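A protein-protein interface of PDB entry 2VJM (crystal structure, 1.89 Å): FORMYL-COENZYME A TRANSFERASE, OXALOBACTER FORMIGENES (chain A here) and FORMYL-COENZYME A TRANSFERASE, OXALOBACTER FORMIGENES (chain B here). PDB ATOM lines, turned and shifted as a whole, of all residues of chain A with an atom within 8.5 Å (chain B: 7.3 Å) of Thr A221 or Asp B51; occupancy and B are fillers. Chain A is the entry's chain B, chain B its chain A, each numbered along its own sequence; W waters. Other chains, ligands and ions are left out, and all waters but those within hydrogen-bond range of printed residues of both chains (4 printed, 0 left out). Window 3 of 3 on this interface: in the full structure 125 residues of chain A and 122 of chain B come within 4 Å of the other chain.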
ATOM      1  N   ARG A 213     -18.111 -18.777  19.771  1.00  0.00           N
ATOM      2  CA  ARG A 213     -17.051 -18.427  18.813  1.00  0.00           C
ATOM      3  C   ARG A 213     -16.280 -19.683  18.402  1.00  0.00           C
ATOM      4  O   ARG A 213     -16.115 -19.961  17.219  1.00  0.00           O
ATOM      5  CB  ARG A 213     -16.090 -17.411  19.439  1.00  0.00           C
ATOM      6  CG  ARG A 213     -14.866 -17.038  18.593  1.00  0.00           C
ATOM      7  CD  ARG A 213     -13.802 -16.382  19.464  1.00  0.00           C
ATOM      8  NE  ARG A 213     -13.023 -17.375  20.207  1.00  0.00           N
ATOM      9  CZ  ARG A 213     -12.441 -17.167  21.389  1.00  0.00           C
ATOM     10  NH1 ARG A 213     -12.547 -15.992  22.018  1.00  0.00           N
ATOM     11  NH2 ARG A 213     -11.751 -18.151  21.962  1.00  0.00           N
ATOM     12  N   ASP A 214     -15.818 -20.439  19.390  1.00  0.00           N
ATOM     13  CA  ASP A 214     -15.020 -21.635  19.125  1.00  0.00           C
ATOM     14  C   ASP A 214     -15.807 -22.726  18.385  1.00  0.00           C
ATOM     15  O   ASP A 214     -15.253 -23.412  17.524  1.00  0.00           O
ATOM     16  CB  ASP A 214     -14.419 -22.180  20.422  1.00  0.00           C
ATOM     17  CG  ASP A 214     -13.371 -21.253  21.014  1.00  0.00           C
ATOM     18  OD1 ASP A 214     -12.945 -20.306  20.325  1.00  0.00           O
ATOM     19  OD2 ASP A 214     -12.971 -21.463  22.174  1.00  0.00           O
ATOM     20  N   GLN A 215     -17.092 -22.873  18.695  1.00  0.00           N
ATOM     21  CA  GLN A 215     -17.921 -23.858  17.995  1.00  0.00           C
ATOM     22  C   GLN A 215     -17.991 -23.570  16.495  1.00  0.00           C
ATOM     23  O   GLN A 215     -17.886 -24.489  15.678  1.00  0.00           O
ATOM     24  CB  GLN A 215     -19.329 -23.929  18.591  1.00  0.00           C
ATOM     25  CG  GLN A 215     -20.218 -25.017  17.966  1.00  0.00           C
ATOM     26  CD  GLN A 215     -19.594 -26.402  18.015  1.00  0.00           C
ATOM     27  OE1 GLN A 215     -18.901 -26.740  18.964  1.00  0.00           O
ATOM     28  NE2 GLN A 215     -19.828 -27.205  16.976  1.00  0.00           N
ATOM     29  N   GLN A 216     -18.166 -22.297  16.148  1.00  0.00           N
ATOM     30  CA  GLN A 216     -18.191 -21.886  14.739  1.00  0.00           C
ATOM     31  C   GLN A 216     -16.834 -22.051  14.069  1.00  0.00           C
ATOM     32  O   GLN A 216     -16.758 -22.552  12.948  1.00  0.00           O
ATOM     33  CB  GLN A 216     -18.690 -20.455  14.601  1.00  0.00           C
ATOM     34  CG  GLN A 216     -20.145 -20.307  14.967  1.00  0.00           C
ATOM     35  CD  GLN A 216     -20.603 -18.872  14.937  1.00  0.00           C
ATOM     36  OE1 GLN A 216     -21.135 -18.405  13.928  1.00  0.00           O
ATOM     37  NE2 GLN A 216     -20.396 -18.152  16.046  1.00  0.00           N
ATOM     38  N   ARG A 217     -15.766 -21.652  14.751  1.00  0.00           N
ATOM     39  CA  ARG A 217     -14.410 -21.910  14.252  1.00  0.00           C
ATOM     40  C   ARG A 217     -14.195 -23.399  13.965  1.00  0.00           C
ATOM     41  O   ARG A 217     -13.645 -23.765  12.921  1.00  0.00           O
ATOM     42  CB  ARG A 217     -13.360 -21.437  15.255  1.00  0.00           C
ATOM     43  CG  ARG A 217     -13.247 -19.924  15.399  1.00  0.00           C
ATOM     44  CD  ARG A 217     -12.377 -19.589  16.583  1.00  0.00           C
ATOM     45  NE  ARG A 217     -11.032 -20.148  16.419  1.00  0.00           N
ATOM     46  CZ  ARG A 217     -10.269 -20.613  17.405  1.00  0.00           C
ATOM     47  NH1 ARG A 217     -10.681 -20.583  18.666  1.00  0.00           N
ATOM     48  NH2 ARG A 217      -9.067 -21.087  17.125  1.00  0.00           N
ATOM     49  N   LEU A 218     -14.634 -24.244  14.896  1.00  0.00           N
ATOM     50  CA  LEU A 218     -14.481 -25.697  14.786  1.00  0.00           C
ATOM     51  C   LEU A 218     -15.267 -26.249  13.595  1.00  0.00           C
ATOM     52  O   LEU A 218     -14.733 -27.040  12.819  1.00  0.00           O
ATOM     53  CB  LEU A 218     -14.934 -26.395  16.081  1.00  0.00           C
ATOM     54  CG  LEU A 218     -14.846 -27.928  16.128  1.00  0.00           C
ATOM     55  CD1 LEU A 218     -13.423 -28.400  15.829  1.00  0.00           C
ATOM     56  CD2 LEU A 218     -15.320 -28.473  17.486  1.00  0.00           C
ATOM     57  N   GLU A 219     -16.529 -25.839  13.469  1.00  0.00           N
ATOM     58  CA  GLU A 219     -17.367 -26.238  12.328  1.00  0.00           C
ATOM     59  C   GLU A 219     -16.786 -25.773  10.988  1.00  0.00           C
ATOM     60  O   GLU A 219     -16.864 -26.488   9.986  1.00  0.00           O
ATOM     61  CB  GLU A 219     -18.797 -25.705  12.496  1.00  0.00           C
ATOM     62  CG  GLU A 219     -19.551 -26.428  13.620  1.00  0.00           C
ATOM     63  CD  GLU A 219     -20.991 -25.979  13.800  1.00  0.00           C
ATOM     64  OE1 GLU A 219     -21.513 -25.221  12.954  1.00  0.00           O
ATOM     65  OE2 GLU A 219     -21.609 -26.399  14.799  1.00  0.00           O
ATOM     66  N   ARG A 220     -16.205 -24.579  10.984  1.00  0.00           N
ATOM     67  CA  ARG A 220     -15.676 -23.968   9.762  1.00  0.00           C
ATOM     68  C   ARG A 220     -14.318 -24.517   9.313  1.00  0.00           C
ATOM     69  O   ARG A 220     -14.035 -24.548   8.109  1.00  0.00           O
ATOM     70  CB  ARG A 220     -15.559 -22.461   9.945  1.00  0.00           C
ATOM     71  CG  ARG A 220     -16.890 -21.743   9.981  1.00  0.00           C
ATOM     72  CD  ARG A 220     -16.674 -20.279  10.211  1.00  0.00           C
ATOM     73  NE  ARG A 220     -17.930 -19.538  10.219  1.00  0.00           N
ATOM     74  CZ  ARG A 220     -18.040 -18.222  10.054  1.00  0.00           C
ATOM     75  NH1 ARG A 220     -16.970 -17.458   9.875  1.00  0.00           N
ATOM     76  NH2 ARG A 220     -19.237 -17.666  10.082  1.00  0.00           N
ATOM     77  N   THR A 221     -13.485 -24.929  10.268  1.00  0.00           N
ATOM     78  CA  THR A 221     -12.080 -25.262   9.995  1.00  0.00           C
ATOM     79  C   THR A 221     -11.644 -26.654  10.451  1.00  0.00           C
ATOM     80  O   THR A 221     -10.578 -27.122  10.047  1.00  0.00           O
ATOM     81  CB  THR A 221     -11.128 -24.242  10.661  1.00  0.00           C
ATOM     82  OG1 THR A 221     -11.060 -24.484  12.077  1.00  0.00           O
ATOM     83  CG2 THR A 221     -11.590 -22.802  10.391  1.00  0.00           C
ATOM     84  N   GLY A 222     -12.436 -27.293  11.310  1.00  0.00           N
ATOM     85  CA  GLY A 222     -12.111 -28.616  11.833  1.00  0.00           C
ATOM     86  C   GLY A 222     -11.048 -28.667  12.920  1.00  0.00           C
ATOM     87  O   GLY A 222     -10.671 -29.758  13.359  1.00  0.00           O
ATOM     88  N   ILE A 223     -10.563 -27.506  13.362  1.00  0.00           N
ATOM     89  CA  ILE A 223      -9.518 -27.438  14.387  1.00  0.00           C
ATOM     90  C   ILE A 223      -9.595 -26.137  15.198  1.00  0.00           C
ATOM     91  O   ILE A 223     -10.040 -25.097  14.697  1.00  0.00           O
ATOM     92  CB  ILE A 223      -8.090 -27.588  13.760  1.00  0.00           C
ATOM     93  CG1 ILE A 223      -7.041 -27.855  14.847  1.00  0.00           C
ATOM     94  CG2 ILE A 223      -7.723 -26.350  12.936  1.00  0.00           C
ATOM     95  CD1 ILE A 223      -5.651 -28.194  14.317  1.00  0.00           C
ATOM     96  N   LEU A 224      -9.188 -26.230  16.463  1.00  0.00           N
ATOM     97  CA  LEU A 224      -8.924 -25.075  17.317  1.00  0.00           C
ATOM     98  C   LEU A 224      -7.465 -25.196  17.747  1.00  0.00           C
ATOM     99  O   LEU A 224      -7.129 -25.990  18.631  1.00  0.00           O
ATOM    100  CB  LEU A 224      -9.842 -25.065  18.543  1.00  0.00           C
ATOM    101  CG  LEU A 224     -11.348 -25.109  18.281  1.00  0.00           C
ATOM    102  CD1 LEU A 224     -12.103 -25.280  19.594  1.00  0.00           C
ATOM    103  CD2 LEU A 224     -11.817 -23.858  17.537  1.00  0.00           C
ATOM    104  N   ALA A 225      -6.602 -24.416  17.105  1.00  0.00           N
ATOM    105  CA  ALA A 225      -5.148 -24.624  17.178  1.00  0.00           C
ATOM    106  C   ALA A 225      -4.541 -24.377  18.563  1.00  0.00           C
ATOM    107  O   ALA A 225      -3.509 -24.972  18.908  1.00  0.00           O
ATOM    108  CB  ALA A 225      -4.443 -23.755  16.125  1.00  0.00           C
ATOM    109  N   PHE A 245      -8.177 -33.193  16.960  1.00  0.00           N
ATOM    110  CA  PHE A 245      -9.467 -32.682  16.508  1.00  0.00           C
ATOM    111  C   PHE A 245     -10.087 -33.491  15.356  1.00  0.00           C
ATOM    112  O   PHE A 245     -11.178 -33.158  14.892  1.00  0.00           O
ATOM    113  CB  PHE A 245      -9.350 -31.196  16.147  1.00  0.00           C
ATOM    114  CG  PHE A 245      -9.440 -30.285  17.336  1.00  0.00           C
ATOM    115  CD1 PHE A 245      -8.296 -29.817  17.964  1.00  0.00           C
ATOM    116  CD2 PHE A 245     -10.682 -29.911  17.843  1.00  0.00           C
ATOM    117  CE1 PHE A 245      -8.386 -28.982  19.069  1.00  0.00           C
ATOM    118  CE2 PHE A 245     -10.777 -29.082  18.949  1.00  0.00           C
ATOM    119  CZ  PHE A 245      -9.634 -28.618  19.562  1.00  0.00           C
ATOM    120  N   ILE A 248     -13.355 -34.610  16.811  1.00  0.00           N
ATOM    121  CA  ILE A 248     -14.029 -33.671  17.716  1.00  0.00           C
ATOM    122  C   ILE A 248     -14.876 -32.696  16.900  1.00  0.00           C
ATOM    123  O   ILE A 248     -14.345 -31.958  16.071  1.00  0.00           O
ATOM    124  CB  ILE A 248     -13.015 -32.889  18.586  1.00  0.00           C
ATOM    125  CG1 ILE A 248     -12.169 -33.852  19.424  1.00  0.00           C
ATOM    126  CG2 ILE A 248     -13.742 -31.897  19.498  1.00  0.00           C
ATOM    127  CD1 ILE A 248     -11.195 -33.157  20.368  1.00  0.00           C
ATOM    128  N   TRP B  48      -7.003 -12.165  15.962  1.00  0.00           N
ATOM    129  CA  TRP B  48      -6.831 -13.285  16.895  1.00  0.00           C
ATOM    130  C   TRP B  48      -7.788 -14.422  16.559  1.00  0.00           C
ATOM    131  O   TRP B  48      -8.993 -14.205  16.485  1.00  0.00           O
ATOM    132  CB  TRP B  48      -7.115 -12.852  18.334  1.00  0.00           C
ATOM    133  CG  TRP B  48      -6.020 -12.093  19.034  1.00  0.00           C
ATOM    134  CD1 TRP B  48      -4.771 -11.790  18.560  1.00  0.00           C
ATOM    135  CD2 TRP B  48      -6.077 -11.579  20.369  1.00  0.00           C
ATOM    136  NE1 TRP B  48      -4.056 -11.093  19.512  1.00  0.00           N
ATOM    137  CE2 TRP B  48      -4.835 -10.953  20.632  1.00  0.00           C
ATOM    138  CE3 TRP B  48      -7.059 -11.577  21.363  1.00  0.00           C
ATOM    139  CZ2 TRP B  48      -4.553 -10.340  21.853  1.00  0.00           C
ATOM    140  CZ3 TRP B  48      -6.783 -10.967  22.572  1.00  0.00           C
ATOM    141  CH2 TRP B  48      -5.539 -10.358  22.811  1.00  0.00           C
ATOM    142  N   LEU B  49      -7.251 -15.632  16.391  1.00  0.00           N
ATOM    143  CA  LEU B  49      -8.062 -16.835  16.184  1.00  0.00           C
ATOM    144  C   LEU B  49      -8.949 -16.739  14.928  1.00  0.00           C
ATOM    145  O   LEU B  49     -10.088 -17.208  14.926  1.00  0.00           O
ATOM    146  CB  LEU B  49      -8.922 -17.123  17.431  1.00  0.00           C
ATOM    147  CG  LEU B  49      -8.223 -17.110  18.806  1.00  0.00           C
ATOM    148  CD1 LEU B  49      -9.232 -17.079  19.959  1.00  0.00           C
ATOM    149  CD2 LEU B  49      -7.296 -18.306  18.953  1.00  0.00           C
ATOM    150  N   GLN B  50      -8.419 -16.135  13.867  1.00  0.00           N
ATOM    151  CA  GLN B  50      -9.155 -15.994  12.608  1.00  0.00           C
ATOM    152  C   GLN B  50      -9.456 -17.370  12.023  1.00  0.00           C
ATOM    153  O   GLN B  50      -8.618 -18.266  12.085  1.00  0.00           O
ATOM    154  CB  GLN B  50      -8.358 -15.174  11.590  1.00  0.00           C
ATOM    155  CG  GLN B  50      -8.265 -13.687  11.892  1.00  0.00           C
ATOM    156  CD  GLN B  50      -7.291 -12.966  10.966  1.00  0.00           C
ATOM    157  OE1 GLN B  50      -6.118 -13.319  10.895  1.00  0.00           O
ATOM    158  NE2 GLN B  50      -7.775 -11.946  10.265  1.00  0.00           N
ATOM    159  N   ASP B  51     -10.653 -17.538  11.474  1.00  0.00           N
ATOM    160  CA  ASP B  51     -11.012 -18.787  10.803  1.00  0.00           C
ATOM    161  C   ASP B  51     -10.741 -18.704   9.296  1.00  0.00           C
ATOM    162  O   ASP B  51     -10.579 -19.729   8.640  1.00  0.00           O
ATOM    163  CB  ASP B  51     -12.473 -19.162  11.070  1.00  0.00           C
ATOM    164  CG  ASP B  51     -13.446 -18.084  10.639  1.00  0.00           C
ATOM    165  OD1 ASP B  51     -13.574 -17.061  11.349  1.00  0.00           O
ATOM    166  OD2 ASP B  51     -14.094 -18.275   9.590  1.00  0.00           O
ATOM    167  N   LYS B  52     -10.702 -17.482   8.767  1.00  0.00           N
ATOM    168  CA  LYS B  52     -10.432 -17.244   7.353  1.00  0.00           C
ATOM    169  C   LYS B  52      -9.318 -16.215   7.227  1.00  0.00           C
ATOM    170  O   LYS B  52      -9.339 -15.189   7.915  1.00  0.00           O
ATOM    171  CB  LYS B  52     -11.679 -16.710   6.655  1.00  0.00           C
ATOM    172  CG  LYS B  52     -11.915 -17.267   5.262  1.00  0.00           C
ATOM    173  CD  LYS B  52     -12.900 -18.421   5.287  1.00  0.00           C
ATOM    174  CE  LYS B  52     -14.329 -17.920   5.402  1.00  0.00           C
ATOM    175  NZ  LYS B  52     -15.254 -18.983   5.861  1.00  0.00           N
ATOM    176  N   PRO B  53      -8.340 -16.472   6.336  1.00  0.00           N
ATOM    177  CA  PRO B  53      -7.331 -15.451   6.097  1.00  0.00           C
ATOM    178  C   PRO B  53      -7.982 -14.207   5.493  1.00  0.00           C
ATOM    179  O   PRO B  53      -8.946 -14.335   4.739  1.00  0.00           O
ATOM    180  CB  PRO B  53      -6.390 -16.111   5.084  1.00  0.00           C
ATOM    181  CG  PRO B  53      -6.724 -17.552   5.071  1.00  0.00           C
ATOM    182  CD  PRO B  53      -8.136 -17.664   5.493  1.00  0.00           C
ATOM    183  N   VAL B  55      -9.890 -12.013   6.899  1.00  0.00           N
ATOM    184  CA  VAL B  55     -11.228 -11.719   7.425  1.00  0.00           C
ATOM    185  C   VAL B  55     -11.162 -11.552   8.945  1.00  0.00           C
ATOM    186  O   VAL B  55     -10.508 -12.339   9.633  1.00  0.00           O
ATOM    187  CB  VAL B  55     -12.250 -12.825   7.062  1.00  0.00           C
ATOM    188  CG1 VAL B  55     -13.647 -12.427   7.485  1.00  0.00           C
ATOM    189  CG2 VAL B  55     -12.227 -13.133   5.557  1.00  0.00           C
ATOM    190  N   ASP B  56     -11.831 -10.521   9.459  1.00  0.00           N
ATOM    191  CA  ASP B  56     -11.905 -10.284  10.903  1.00  0.00           C
ATOM    192  C   ASP B  56     -12.396 -11.548  11.594  1.00  0.00           C
ATOM    193  O   ASP B  56     -13.339 -12.188  11.122  1.00  0.00           O
ATOM    194  CB  ASP B  56     -12.870  -9.143  11.230  1.00  0.00           C
ATOM    195  CG  ASP B  56     -12.359  -7.790  10.776  1.00  0.00           C
ATOM    196  OD1 ASP B  56     -11.170  -7.497  10.981  1.00  0.00           O
ATOM    197  OD2 ASP B  56     -13.159  -7.001  10.242  1.00  0.00           O
ATOM    198  N   SER B  57     -11.758 -11.900  12.704  1.00  0.00           N
ATOM    199  CA  SER B  57     -12.096 -13.127  13.426  1.00  0.00           C
ATOM    200  C   SER B  57     -13.501 -13.080  14.012  1.00  0.00           C
ATOM    201  O   SER B  57     -14.091 -12.012  14.159  1.00  0.00           O
ATOM    202  CB  SER B  57     -11.093 -13.390  14.553  1.00  0.00           C
ATOM    203  OG  SER B  57     -11.242 -12.444  15.599  1.00  0.00           O
ATOM    204  N   LEU B  58     -14.017 -14.254  14.362  1.00  0.00           N
ATOM    205  CA  LEU B  58     -15.272 -14.351  15.092  1.00  0.00           C
ATOM    206  C   LEU B  58     -15.113 -13.765  16.498  1.00  0.00           C
ATOM    207  O   LEU B  58     -16.094 -13.314  17.089  1.00  0.00           O
ATOM    208  CB  LEU B  58     -15.757 -15.795  15.161  1.00  0.00           C
ATOM    209  CG  LEU B  58     -16.290 -16.339  13.827  1.00  0.00           C
ATOM    210  CD1 LEU B  58     -16.204 -17.850  13.771  1.00  0.00           C
ATOM    211  CD2 LEU B  58     -17.719 -15.858  13.594  1.00  0.00           C
ATOM    212  N   TYR B  59     -13.888 -13.775  17.026  1.00  0.00           N
ATOM    213  CA  TYR B  59     -13.611 -13.107  18.302  1.00  0.00           C
ATOM    214  C   TYR B  59     -14.007 -11.631  18.180  1.00  0.00           C
ATOM    215  O   TYR B  59     -14.707 -11.088  19.035  1.00  0.00           O
ATOM    216  CB  TYR B  59     -12.134 -13.232  18.708  1.00  0.00           C
ATOM    217  CG  TYR B  59     -11.842 -13.011  20.195  1.00  0.00           C
ATOM    218  CD1 TYR B  59     -10.589 -13.310  20.722  1.00  0.00           C
ATOM    219  CD2 TYR B  59     -12.818 -12.516  21.074  1.00  0.00           C
ATOM    220  CE1 TYR B  59     -10.309 -13.119  22.079  1.00  0.00           C
ATOM    221  CE2 TYR B  59     -12.541 -12.321  22.427  1.00  0.00           C
ATOM    222  CZ  TYR B  59     -11.290 -12.621  22.922  1.00  0.00           C
ATOM    223  OH  TYR B  59     -11.029 -12.422  24.270  1.00  0.00           O
ATOM    224  N   THR B  61     -15.999 -10.182  15.618  1.00  0.00           N
ATOM    225  CA  THR B  61     -17.360  -9.911  15.137  1.00  0.00           C
ATOM    226  C   THR B  61     -18.430 -10.171  16.212  1.00  0.00           C
ATOM    227  O   THR B  61     -19.398  -9.429  16.318  1.00  0.00           O
ATOM    228  CB  THR B  61     -17.689 -10.683  13.837  1.00  0.00           C
ATOM    229  OG1 THR B  61     -17.621 -12.093  14.063  1.00  0.00           O
ATOM    230  CG2 THR B  61     -16.712 -10.290  12.729  1.00  0.00           C
ATOM    231  N   ARG B 376     -18.423 -10.825   5.290  1.00  0.00           N
ATOM    232  CA  ARG B 376     -17.707 -11.954   5.902  1.00  0.00           C
ATOM    233  C   ARG B 376     -18.478 -13.273   5.848  1.00  0.00           C
ATOM    234  O   ARG B 376     -17.943 -14.319   6.219  1.00  0.00           O
ATOM    235  CB  ARG B 376     -17.403 -11.632   7.367  1.00  0.00           C
ATOM    236  CG  ARG B 376     -16.768 -10.271   7.599  1.00  0.00           C
ATOM    237  CD  ARG B 376     -16.455 -10.097   9.071  1.00  0.00           C
ATOM    238  NE  ARG B 376     -15.906  -8.780   9.403  1.00  0.00           N
ATOM    239  CZ  ARG B 376     -16.620  -7.721   9.781  1.00  0.00           C
ATOM    240  NH1 ARG B 376     -17.942  -7.786   9.869  1.00  0.00           N
ATOM    241  NH2 ARG B 376     -16.003  -6.583  10.079  1.00  0.00           N
HETATM  242  O   HOH W   1     -18.646 -14.704   9.476  1.00  0.00           O
HETATM  243  O   HOH W   2      -9.973 -20.492  13.731  1.00  0.00           O
HETATM  244  O   HOH W   3     -15.799 -15.233   7.888  1.00  0.00           O
HETATM  245  O   HOH W   4     -11.213 -15.362  24.909  1.00  0.00           O
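Printed residues of chain B within 4 Å of Arg A213: Leu B49 (3.4 Å), Leu B58 (3.8 Å) and Tyr B59 (3.5 Å). Of the printed residues of chain B, Gln A216 touches Leu B58 (3.7 Å). Of the printed residues of chain B, Arg A217 touches Leu B49 and Leu B58. Of the printed residues of chain B, Arg A220 touches Asp B51 and Leu B58. Thr A221 touches just one residue of chain B: Asp B51. Of the printed residues of chain A, Asp B51 touches Arg A220 and Thr A221. No residue of chain A comes within 4 Å of Lys B52. Of the printed residues of chain A, Tyr B59 touches Arg A213. The nearest printed residue of chain B that does not touch Arg A220 is Lys B52 (4.6 Å).
OD2 of Asp B51 lies within salt-bridge range of NZ of Lys B52, at 3.97 Å. The side-chain hydroxyl of Ser B57 sits close to the backbone NH of Tyr B59 (3.3 Å). The guanidinium group (NE) of Arg A213 lies within salt-bridge range of the side-chain carboxylate (OD1) of Asp A214, at 2.9 Å. The side-chain carboxylate of Asp A214 is in salt-bridge range of the guanidinium group of Arg A217 (2.8 Å). O of Arg A217 lies within hydrogen-bond range of OG1 of Thr A221 (2.8 Å). The backbone carbonyl oxygen of Ile A223 sits at hydrogen-bond distance from the side-chain hydroxyl of Thr A221 (2.9 Å).
The backbone carbonyl oxygen (O) of Leu B49 is in hydrogen-bond range of the guanidinium group (NE) of Arg A217, 3.4 Å away. OD2 of Asp B51 is in salt-bridge range of NH1 of Arg A220, 3.0 Å away.
Water W3 bridges the backbone carbonyl oxygen (O) of Arg B376 (2.9 Å) and the guanidinium group (NH1) of Arg A220 (3.2 Å). Water W2 lies within hydrogen-bond range of NE of Arg A217 (2.9 Å), O of Gln B50 (3.1 Å) and O of Leu B49 (3.5 Å). Water W4 lies within hydrogen-bond range of the side-chain hydroxyl of Tyr B59 (3.0 Å) and the guanidinium group of Arg A213 (3.2 Å). Water W1 lies within hydrogen-bond range of NH2 of Arg A220 and O of Arg B376.
Of the 13 printed residues of chain B, 4 touch a printed residue of chain A. Printed residues of chain B that touch a printed residue of chain A: Leu B49, Asp B51, Leu B58 and Tyr B59. Hydrophobic or aromatic side chains of chain B within 4 Å of the printed part of chain A: Leu B49, Leu B58 and Tyr B59. Along chain A the printed residues that touch a printed residue of chain B span positions 213 to 221. Among the printed residues, 9 pairs touch across the chains. Among the printed residues, Asp or Glu carboxylates within 4 Å of a Lys or Arg side-chain nitrogen of the other chain: Arg A220 with Asp B51 (3.0 Å).
Arg A213 touches Leu B49. CG of Arg A213 touches CB of Leu B58, 3.8 Å away. Arg A213 touches Tyr B59. CD1 of Leu B58 touches CB of Gln A216, at 3.7 Å. N of Arg A217 touches CD1 of Leu B58, at 3.95 Å. NH1 of Arg A220 touches CD1 of Leu B58, at 3.99 Å. Thr A221 touches Asp B51 (CG2 to O, 3.7 Å).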
